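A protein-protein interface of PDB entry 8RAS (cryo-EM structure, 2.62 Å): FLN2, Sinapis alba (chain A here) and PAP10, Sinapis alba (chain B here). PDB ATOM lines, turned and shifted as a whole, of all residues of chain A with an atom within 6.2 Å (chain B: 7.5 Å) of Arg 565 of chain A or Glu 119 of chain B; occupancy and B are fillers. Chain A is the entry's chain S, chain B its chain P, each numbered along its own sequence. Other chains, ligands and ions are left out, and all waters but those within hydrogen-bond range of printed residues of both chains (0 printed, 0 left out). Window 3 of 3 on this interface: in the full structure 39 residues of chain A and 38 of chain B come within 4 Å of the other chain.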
ATOM      1  N   PHE A 483      -1.710  -1.725  13.150  1.00  0.00           N
ATOM      2  CA  PHE A 483      -1.473  -0.310  12.906  1.00  0.00           C
ATOM      3  C   PHE A 483      -0.547  -0.052  11.725  1.00  0.00           C
ATOM      4  O   PHE A 483      -0.456   1.094  11.273  1.00  0.00           O
ATOM      5  CB  PHE A 483      -0.887   0.349  14.158  1.00  0.00           C
ATOM      6  CG  PHE A 483      -1.856   0.452  15.301  1.00  0.00           C
ATOM      7  CD1 PHE A 483      -3.219   0.499  15.070  1.00  0.00           C
ATOM      8  CD2 PHE A 483      -1.401   0.513  16.606  1.00  0.00           C
ATOM      9  CE1 PHE A 483      -4.108   0.597  16.121  1.00  0.00           C
ATOM     10  CE2 PHE A 483      -2.285   0.610  17.658  1.00  0.00           C
ATOM     11  CZ  PHE A 483      -3.640   0.654  17.416  1.00  0.00           C
ATOM     12  N   TYR A 539       1.205  -2.974  18.826  1.00  0.00           N
ATOM     13  CA  TYR A 539      -0.070  -3.615  18.542  1.00  0.00           C
ATOM     14  C   TYR A 539      -1.211  -2.944  19.300  1.00  0.00           C
ATOM     15  O   TYR A 539      -1.007  -2.395  20.387  1.00  0.00           O
ATOM     16  CB  TYR A 539      -0.020  -5.091  18.925  1.00  0.00           C
ATOM     17  CG  TYR A 539       0.937  -5.920  18.105  1.00  0.00           C
ATOM     18  CD1 TYR A 539       2.298  -5.906  18.368  1.00  0.00           C
ATOM     19  CD2 TYR A 539       0.477  -6.725  17.074  1.00  0.00           C
ATOM     20  CE1 TYR A 539       3.175  -6.665  17.625  1.00  0.00           C
ATOM     21  CE2 TYR A 539       1.347  -7.487  16.326  1.00  0.00           C
ATOM     22  CZ  TYR A 539       2.694  -7.454  16.605  1.00  0.00           C
ATOM     23  OH  TYR A 539       3.565  -8.213  15.861  1.00  0.00           O
ATOM     24  N   PRO A 540      -2.425  -2.978  18.744  1.00  0.00           N
ATOM     25  CA  PRO A 540      -3.588  -2.554  19.517  1.00  0.00           C
ATOM     26  C   PRO A 540      -3.869  -3.537  20.637  1.00  0.00           C
ATOM     27  O   PRO A 540      -3.564  -4.736  20.519  1.00  0.00           O
ATOM     28  CB  PRO A 540      -4.721  -2.546  18.475  1.00  0.00           C
ATOM     29  CG  PRO A 540      -4.268  -3.474  17.416  1.00  0.00           C
ATOM     30  CD  PRO A 540      -2.777  -3.353  17.365  1.00  0.00           C
ATOM     31  N   PRO A 541      -4.458  -3.078  21.750  1.00  0.00           N
ATOM     32  CA  PRO A 541      -4.737  -3.962  22.883  1.00  0.00           C
ATOM     33  C   PRO A 541      -5.986  -4.809  22.668  1.00  0.00           C
ATOM     34  O   PRO A 541      -5.900  -6.033  22.768  1.00  0.00           O
ATOM     35  CB  PRO A 541      -4.933  -2.987  24.042  1.00  0.00           C
ATOM     36  CG  PRO A 541      -5.467  -1.757  23.400  1.00  0.00           C
ATOM     37  CD  PRO A 541      -4.908  -1.698  22.001  1.00  0.00           C
ATOM     38  N   GLY A 563      -6.982   9.459  22.309  1.00  0.00           N
ATOM     39  CA  GLY A 563      -7.138   8.135  22.869  1.00  0.00           C
ATOM     40  C   GLY A 563      -6.555   7.074  21.962  1.00  0.00           C
ATOM     41  O   GLY A 563      -7.216   6.604  21.032  1.00  0.00           O
ATOM     42  N   ILE A 564      -5.311   6.687  22.235  1.00  0.00           N
ATOM     43  CA  ILE A 564      -4.592   5.707  21.431  1.00  0.00           C
ATOM     44  C   ILE A 564      -3.804   4.832  22.394  1.00  0.00           C
ATOM     45  O   ILE A 564      -2.817   5.286  22.984  1.00  0.00           O
ATOM     46  CB  ILE A 564      -3.657   6.359  20.400  1.00  0.00           C
ATOM     47  CG1 ILE A 564      -4.472   7.006  19.279  1.00  0.00           C
ATOM     48  CG2 ILE A 564      -2.700   5.331  19.819  1.00  0.00           C
ATOM     49  CD1 ILE A 564      -3.791   8.181  18.632  1.00  0.00           C
ATOM     50  N   ARG A 565      -4.243   3.591  22.568  1.00  0.00           N
ATOM     51  CA  ARG A 565      -3.567   2.627  23.419  1.00  0.00           C
ATOM     52  C   ARG A 565      -2.900   1.580  22.541  1.00  0.00           C
ATOM     53  O   ARG A 565      -3.518   1.069  21.602  1.00  0.00           O
ATOM     54  CB  ARG A 565      -4.547   1.964  24.387  1.00  0.00           C
ATOM     55  CG  ARG A 565      -5.303   2.942  25.269  1.00  0.00           C
ATOM     56  CD  ARG A 565      -6.609   2.339  25.752  1.00  0.00           C
ATOM     57  NE  ARG A 565      -7.290   1.603  24.695  1.00  0.00           N
ATOM     58  CZ  ARG A 565      -8.022   2.162  23.742  1.00  0.00           C
ATOM     59  NH1 ARG A 565      -8.198   3.472  23.686  1.00  0.00           N
ATOM     60  NH2 ARG A 565      -8.594   1.389  22.824  1.00  0.00           N
ATOM     61  N   SER A 566      -1.640   1.280  22.834  1.00  0.00           N
ATOM     62  CA  SER A 566      -0.899   0.274  22.092  1.00  0.00           C
ATOM     63  C   SER A 566      -0.111  -0.588  23.064  1.00  0.00           C
ATOM     64  O   SER A 566       0.268  -0.141  24.150  1.00  0.00           O
ATOM     65  CB  SER A 566       0.044   0.910  21.061  1.00  0.00           C
ATOM     66  OG  SER A 566       1.319   1.163  21.621  1.00  0.00           O
ATOM     67  N   ILE A 567       0.129  -1.833  22.663  1.00  0.00           N
ATOM     68  CA  ILE A 567       0.928  -2.766  23.441  1.00  0.00           C
ATOM     69  C   ILE A 567       2.126  -3.188  22.602  1.00  0.00           C
ATOM     70  O   ILE A 567       2.100  -3.148  21.370  1.00  0.00           O
ATOM     71  CB  ILE A 567       0.116  -3.995  23.898  1.00  0.00           C
ATOM     72  CG1 ILE A 567      -0.357  -4.807  22.692  1.00  0.00           C
ATOM     73  CG2 ILE A 567      -1.067  -3.564  24.744  1.00  0.00           C
ATOM     74  CD1 ILE A 567      -1.194  -6.007  23.055  1.00  0.00           C
ATOM     75  N   LEU B  78     -19.983   5.058  20.408  1.00  0.00           N
ATOM     76  CA  LEU B  78     -20.299   3.942  19.524  1.00  0.00           C
ATOM     77  C   LEU B  78     -20.405   4.401  18.074  1.00  0.00           C
ATOM     78  O   LEU B  78     -21.176   5.304  17.753  1.00  0.00           O
ATOM     79  CB  LEU B  78     -21.601   3.265  19.957  1.00  0.00           C
ATOM     80  CG  LEU B  78     -21.467   1.998  20.805  1.00  0.00           C
ATOM     81  CD1 LEU B  78     -20.904   0.853  19.976  1.00  0.00           C
ATOM     82  CD2 LEU B  78     -20.602   2.252  22.030  1.00  0.00           C
ATOM     83  N   VAL B  79     -19.624   3.769  17.200  1.00  0.00           N
ATOM     84  CA  VAL B  79     -19.613   4.071  15.774  1.00  0.00           C
ATOM     85  C   VAL B  79     -20.243   2.898  15.038  1.00  0.00           C
ATOM     86  O   VAL B  79     -19.835   1.745  15.229  1.00  0.00           O
ATOM     87  CB  VAL B  79     -18.188   4.347  15.268  1.00  0.00           C
ATOM     88  CG1 VAL B  79     -18.228   5.020  13.909  1.00  0.00           C
ATOM     89  CG2 VAL B  79     -17.431   5.208  16.266  1.00  0.00           C
ATOM     90  N   LEU B 113      -6.298   3.548  14.066  1.00  0.00           N
ATOM     91  CA  LEU B 113      -5.970   4.615  15.009  1.00  0.00           C
ATOM     92  C   LEU B 113      -7.062   5.682  15.039  1.00  0.00           C
ATOM     93  O   LEU B 113      -7.440   6.173  16.112  1.00  0.00           O
ATOM     94  CB  LEU B 113      -4.617   5.228  14.650  1.00  0.00           C
ATOM     95  CG  LEU B 113      -3.408   4.299  14.797  1.00  0.00           C
ATOM     96  CD1 LEU B 113      -2.231   4.793  13.971  1.00  0.00           C
ATOM     97  CD2 LEU B 113      -3.018   4.154  16.258  1.00  0.00           C
ATOM     98  N   MET B 114      -7.588   6.045  13.867  1.00  0.00           N
ATOM     99  CA  MET B 114      -8.701   6.985  13.804  1.00  0.00           C
ATOM    100  C   MET B 114      -9.951   6.406  14.444  1.00  0.00           C
ATOM    101  O   MET B 114     -10.746   7.146  15.026  1.00  0.00           O
ATOM    102  CB  MET B 114      -8.977   7.373  12.351  1.00  0.00           C
ATOM    103  CG  MET B 114     -10.036   8.449  12.184  1.00  0.00           C
ATOM    104  SD  MET B 114      -9.714   9.892  13.212  1.00  0.00           S
ATOM    105  CE  MET B 114      -8.708  10.873  12.104  1.00  0.00           C
ATOM    106  N   ALA B 115     -10.151   5.091  14.337  1.00  0.00           N
ATOM    107  CA  ALA B 115     -11.274   4.455  15.016  1.00  0.00           C
ATOM    108  C   ALA B 115     -11.144   4.584  16.526  1.00  0.00           C
ATOM    109  O   ALA B 115     -12.130   4.849  17.221  1.00  0.00           O
ATOM    110  CB  ALA B 115     -11.373   2.987  14.606  1.00  0.00           C
ATOM    111  N   GLN B 116      -9.933   4.395  17.053  1.00  0.00           N
ATOM    112  CA  GLN B 116      -9.716   4.594  18.485  1.00  0.00           C
ATOM    113  C   GLN B 116      -9.986   6.041  18.888  1.00  0.00           C
ATOM    114  O   GLN B 116     -10.643   6.303  19.908  1.00  0.00           O
ATOM    115  CB  GLN B 116      -8.291   4.195  18.865  1.00  0.00           C
ATOM    116  CG  GLN B 116      -8.059   2.699  18.954  1.00  0.00           C
ATOM    117  CD  GLN B 116      -6.641   2.360  19.366  1.00  0.00           C
ATOM    118  OE1 GLN B 116      -5.774   3.230  19.418  1.00  0.00           O
ATOM    119  NE2 GLN B 116      -6.399   1.091  19.664  1.00  0.00           N
ATOM    120  N   GLU B 117      -9.488   6.993  18.094  1.00  0.00           N
ATOM    121  CA  GLU B 117      -9.729   8.403  18.391  1.00  0.00           C
ATOM    122  C   GLU B 117     -11.219   8.728  18.360  1.00  0.00           C
ATOM    123  O   GLU B 117     -11.725   9.447  19.229  1.00  0.00           O
ATOM    124  CB  GLU B 117      -8.968   9.287  17.403  1.00  0.00           C
ATOM    125  CG  GLU B 117      -7.518   9.534  17.776  1.00  0.00           C
ATOM    126  CD  GLU B 117      -6.862  10.586  16.902  1.00  0.00           C
ATOM    127  OE1 GLU B 117      -7.126  10.598  15.683  1.00  0.00           O
ATOM    128  OE2 GLU B 117      -6.082  11.403  17.435  1.00  0.00           O
ATOM    129  N   LEU B 118     -11.935   8.199  17.367  1.00  0.00           N
ATOM    130  CA  LEU B 118     -13.366   8.450  17.250  1.00  0.00           C
ATOM    131  C   LEU B 118     -14.142   7.797  18.385  1.00  0.00           C
ATOM    132  O   LEU B 118     -15.148   8.343  18.844  1.00  0.00           O
ATOM    133  CB  LEU B 118     -13.873   7.953  15.899  1.00  0.00           C
ATOM    134  CG  LEU B 118     -13.618   8.880  14.714  1.00  0.00           C
ATOM    135  CD1 LEU B 118     -13.891   8.160  13.411  1.00  0.00           C
ATOM    136  CD2 LEU B 118     -14.486  10.116  14.828  1.00  0.00           C
ATOM    137  N   GLU B 119     -13.706   6.620  18.836  1.00  0.00           N
ATOM    138  CA  GLU B 119     -14.359   5.986  19.976  1.00  0.00           C
ATOM    139  C   GLU B 119     -14.187   6.830  21.233  1.00  0.00           C
ATOM    140  O   GLU B 119     -15.146   7.037  21.990  1.00  0.00           O
ATOM    141  CB  GLU B 119     -13.804   4.575  20.177  1.00  0.00           C
ATOM    142  CG  GLU B 119     -13.593   4.168  21.624  1.00  0.00           C
ATOM    143  CD  GLU B 119     -12.811   2.874  21.753  1.00  0.00           C
ATOM    144  OE1 GLU B 119     -13.395   1.799  21.503  1.00  0.00           O
ATOM    145  OE2 GLU B 119     -11.614   2.934  22.104  1.00  0.00           O
ATOM    146  N   MET B 120     -12.980   7.355  21.456  1.00  0.00           N
ATOM    147  CA  MET B 120     -12.789   8.251  22.592  1.00  0.00           C
ATOM    148  C   MET B 120     -13.651   9.501  22.454  1.00  0.00           C
ATOM    149  O   MET B 120     -14.270   9.947  23.427  1.00  0.00           O
ATOM    150  CB  MET B 120     -11.315   8.625  22.742  1.00  0.00           C
ATOM    151  CG  MET B 120     -11.092   9.909  23.526  1.00  0.00           C
ATOM    152  SD  MET B 120      -9.665   9.841  24.625  1.00  0.00           S
ATOM    153  CE  MET B 120      -9.433  11.578  24.998  1.00  0.00           C
ATOM    154  N   LEU B 121     -13.722  10.067  21.246  1.00  0.00           N
ATOM    155  CA  LEU B 121     -14.534  11.261  21.025  1.00  0.00           C
ATOM    156  C   LEU B 121     -16.011  10.989  21.292  1.00  0.00           C
ATOM    157  O   LEU B 121     -16.699  11.809  21.912  1.00  0.00           O
ATOM    158  CB  LEU B 121     -14.334  11.769  19.598  1.00  0.00           C
ATOM    159  CG  LEU B 121     -15.073  13.047  19.200  1.00  0.00           C
ATOM    160  CD1 LEU B 121     -14.434  14.260  19.849  1.00  0.00           C
ATOM    161  CD2 LEU B 121     -15.097  13.197  17.688  1.00  0.00           C
ATOM    162  N   ALA B 122     -16.516   9.845  20.827  1.00  0.00           N
ATOM    163  CA  ALA B 122     -17.901   9.475  21.088  1.00  0.00           C
ATOM    164  C   ALA B 122     -18.144   9.257  22.572  1.00  0.00           C
ATOM    165  O   ALA B 122     -19.258   9.479  23.059  1.00  0.00           O
ATOM    166  CB  ALA B 122     -18.273   8.221  20.297  1.00  0.00           C
ATOM    167  N   VAL B 123     -17.125   8.805  23.304  1.00  0.00           N
ATOM    168  CA  VAL B 123     -17.235   8.778  24.760  1.00  0.00           C
ATOM    169  C   VAL B 123     -17.370  10.197  25.303  1.00  0.00           C
ATOM    170  O   VAL B 123     -18.195  10.466  26.186  1.00  0.00           O
ATOM    171  CB  VAL B 123     -16.035   8.037  25.376  1.00  0.00           C
ATOM    172  CG1 VAL B 123     -15.824   8.461  26.823  1.00  0.00           C
ATOM    173  CG2 VAL B 123     -16.241   6.533  25.283  1.00  0.00           C
ATOM    174  N   GLU B 124     -16.570  11.131  24.778  1.00  0.00           N
ATOM    175  CA  GLU B 124     -16.666  12.522  25.218  1.00  0.00           C
ATOM    176  C   GLU B 124     -17.990  13.156  24.802  1.00  0.00           C
ATOM    177  O   GLU B 124     -18.563  13.950  25.555  1.00  0.00           O
ATOM    178  CB  GLU B 124     -15.492  13.341  24.679  1.00  0.00           C
ATOM    179  CG  GLU B 124     -14.143  12.657  24.787  1.00  0.00           C
ATOM    180  CD  GLU B 124     -13.171  13.421  25.661  1.00  0.00           C
ATOM    181  OE1 GLU B 124     -13.292  14.660  25.747  1.00  0.00           O
ATOM    182  OE2 GLU B 124     -12.284  12.780  26.265  1.00  0.00           O
ATOM    183  N   TYR B 125     -18.478  12.842  23.605  1.00  0.00           N
ATOM    184  CA  TYR B 125     -19.752  13.359  23.103  1.00  0.00           C
ATOM    185  C   TYR B 125     -20.769  12.219  23.160  1.00  0.00           C
ATOM    186  O   TYR B 125     -20.968  11.496  22.182  1.00  0.00           O
ATOM    187  CB  TYR B 125     -19.604  13.910  21.686  1.00  0.00           C
ATOM    188  CG  TYR B 125     -18.880  15.237  21.607  1.00  0.00           C
ATOM    189  CD1 TYR B 125     -19.250  16.302  22.418  1.00  0.00           C
ATOM    190  CD2 TYR B 125     -17.828  15.423  20.723  1.00  0.00           C
ATOM    191  CE1 TYR B 125     -18.591  17.515  22.347  1.00  0.00           C
ATOM    192  CE2 TYR B 125     -17.163  16.631  20.646  1.00  0.00           C
ATOM    193  CZ  TYR B 125     -17.548  17.673  21.459  1.00  0.00           C
ATOM    194  OH  TYR B 125     -16.887  18.877  21.384  1.00  0.00           O
ATOM    195  N   ILE B 131     -21.405   9.733  15.422  1.00  0.00           N
ATOM    196  CA  ILE B 131     -20.236   9.311  14.659  1.00  0.00           C
ATOM    197  C   ILE B 131     -20.577   8.006  13.957  1.00  0.00           C
ATOM    198  O   ILE B 131     -20.985   7.034  14.605  1.00  0.00           O
ATOM    199  CB  ILE B 131     -18.996   9.146  15.550  1.00  0.00           C
ATOM    200  CG1 ILE B 131     -18.649  10.471  16.230  1.00  0.00           C
ATOM    201  CG2 ILE B 131     -17.823   8.638  14.733  1.00  0.00           C
ATOM    202  CD1 ILE B 131     -17.678  10.332  17.376  1.00  0.00           C
ATOM    203  N   LEU B 174      -7.414  14.920  18.292  1.00  0.00           N
ATOM    204  CA  LEU B 174      -8.753  15.112  18.841  1.00  0.00           C
ATOM    205  C   LEU B 174      -9.075  16.585  19.058  1.00  0.00           C
ATOM    206  O   LEU B 174     -10.244  16.982  18.966  1.00  0.00           O
ATOM    207  CB  LEU B 174      -8.888  14.346  20.154  1.00  0.00           C
ATOM    208  CG  LEU B 174      -9.493  12.949  20.060  1.00  0.00           C
ATOM    209  CD1 LEU B 174      -9.407  12.255  21.400  1.00  0.00           C
ATOM    210  CD2 LEU B 174     -10.931  13.026  19.591  1.00  0.00           C
ATOM    211  N   MET B 177     -10.695  18.045  16.105  1.00  0.00           N
ATOM    212  CA  MET B 177     -12.082  17.600  16.040  1.00  0.00           C
ATOM    213  C   MET B 177     -12.966  18.452  16.944  1.00  0.00           C
ATOM    214  O   MET B 177     -14.029  18.936  16.528  1.00  0.00           O
ATOM    215  CB  MET B 177     -12.156  16.132  16.455  1.00  0.00           C
ATOM    216  CG  MET B 177     -11.805  15.145  15.362  1.00  0.00           C
ATOM    217  SD  MET B 177     -10.993  13.698  16.068  1.00  0.00           S
ATOM    218  CE  MET B 177     -11.786  12.374  15.173  1.00  0.00           C
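Phe 483 of chain A touches Leu 113 of chain B. Phe 483 of chain A touches Gln 116 of chain B. CD of Pro 541 of chain A touches NE2 of Gln 116 of chain B, at 3.9 Å. Gly 563 of chain A touches Gln 116 of chain B. Gly 563 of chain A touches Glu 117 of chain B. Gly 563 of chain A touches Leu 174 of chain B. Ile 564 of chain A touches Leu 113 of chain B. Ile 564 of chain A touches Gln 116 of chain B.
The side-chain amide nitrogen (NE2) of Gln 116 of chain B lies within hydrogen-bond range of the backbone carbonyl oxygen (O) of Arg 565 of chain A (3.5 Å). The side-chain carboxylate of Glu 119 of chain B is in salt-bridge range of the guanidinium group of Arg 565 of chain A (3.5 Å). The backbone NH of Gly 563 of chain A sits close to the side-chain sulfur of Met 120 of chain B (3.6 Å).
Printed residues of chain B that touch a printed residue of chain A: Leu 113, Gln 116, Glu 117, Glu 119, Met 120 and Leu 174. Hydrophobic or aromatic side chains of chain B within 4 Å of the printed part of chain A: Leu 113, Met 120 and Leu 174. Among the printed residues, 11 pairs touch across the chains. Among the printed residues, Asp or Glu carboxylates within 4 Å of a Lys or Arg side-chain nitrogen of the other chain: Arg 565 of chain A with Glu 119 of chain B.
Of the printed residues of chain B, Phe 483 of chain A touches Leu 113 and Gln 116. Of the printed residues of chain B, Pro 541 of chain A touches Gln 116. Ser 566 of chain A touches none of the printed residues of chain B. Printed residues of chain A within 4 Å of Gln 116 of chain B: Phe 483, Pro 541, Gly 563, Ile 564 and Arg 565. Of chain A, only Arg 565 (3.5 Å) comes within 4 Å of Glu 119 of chain B. Leu 121 of chain B touches none of the printed residues of chain A.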
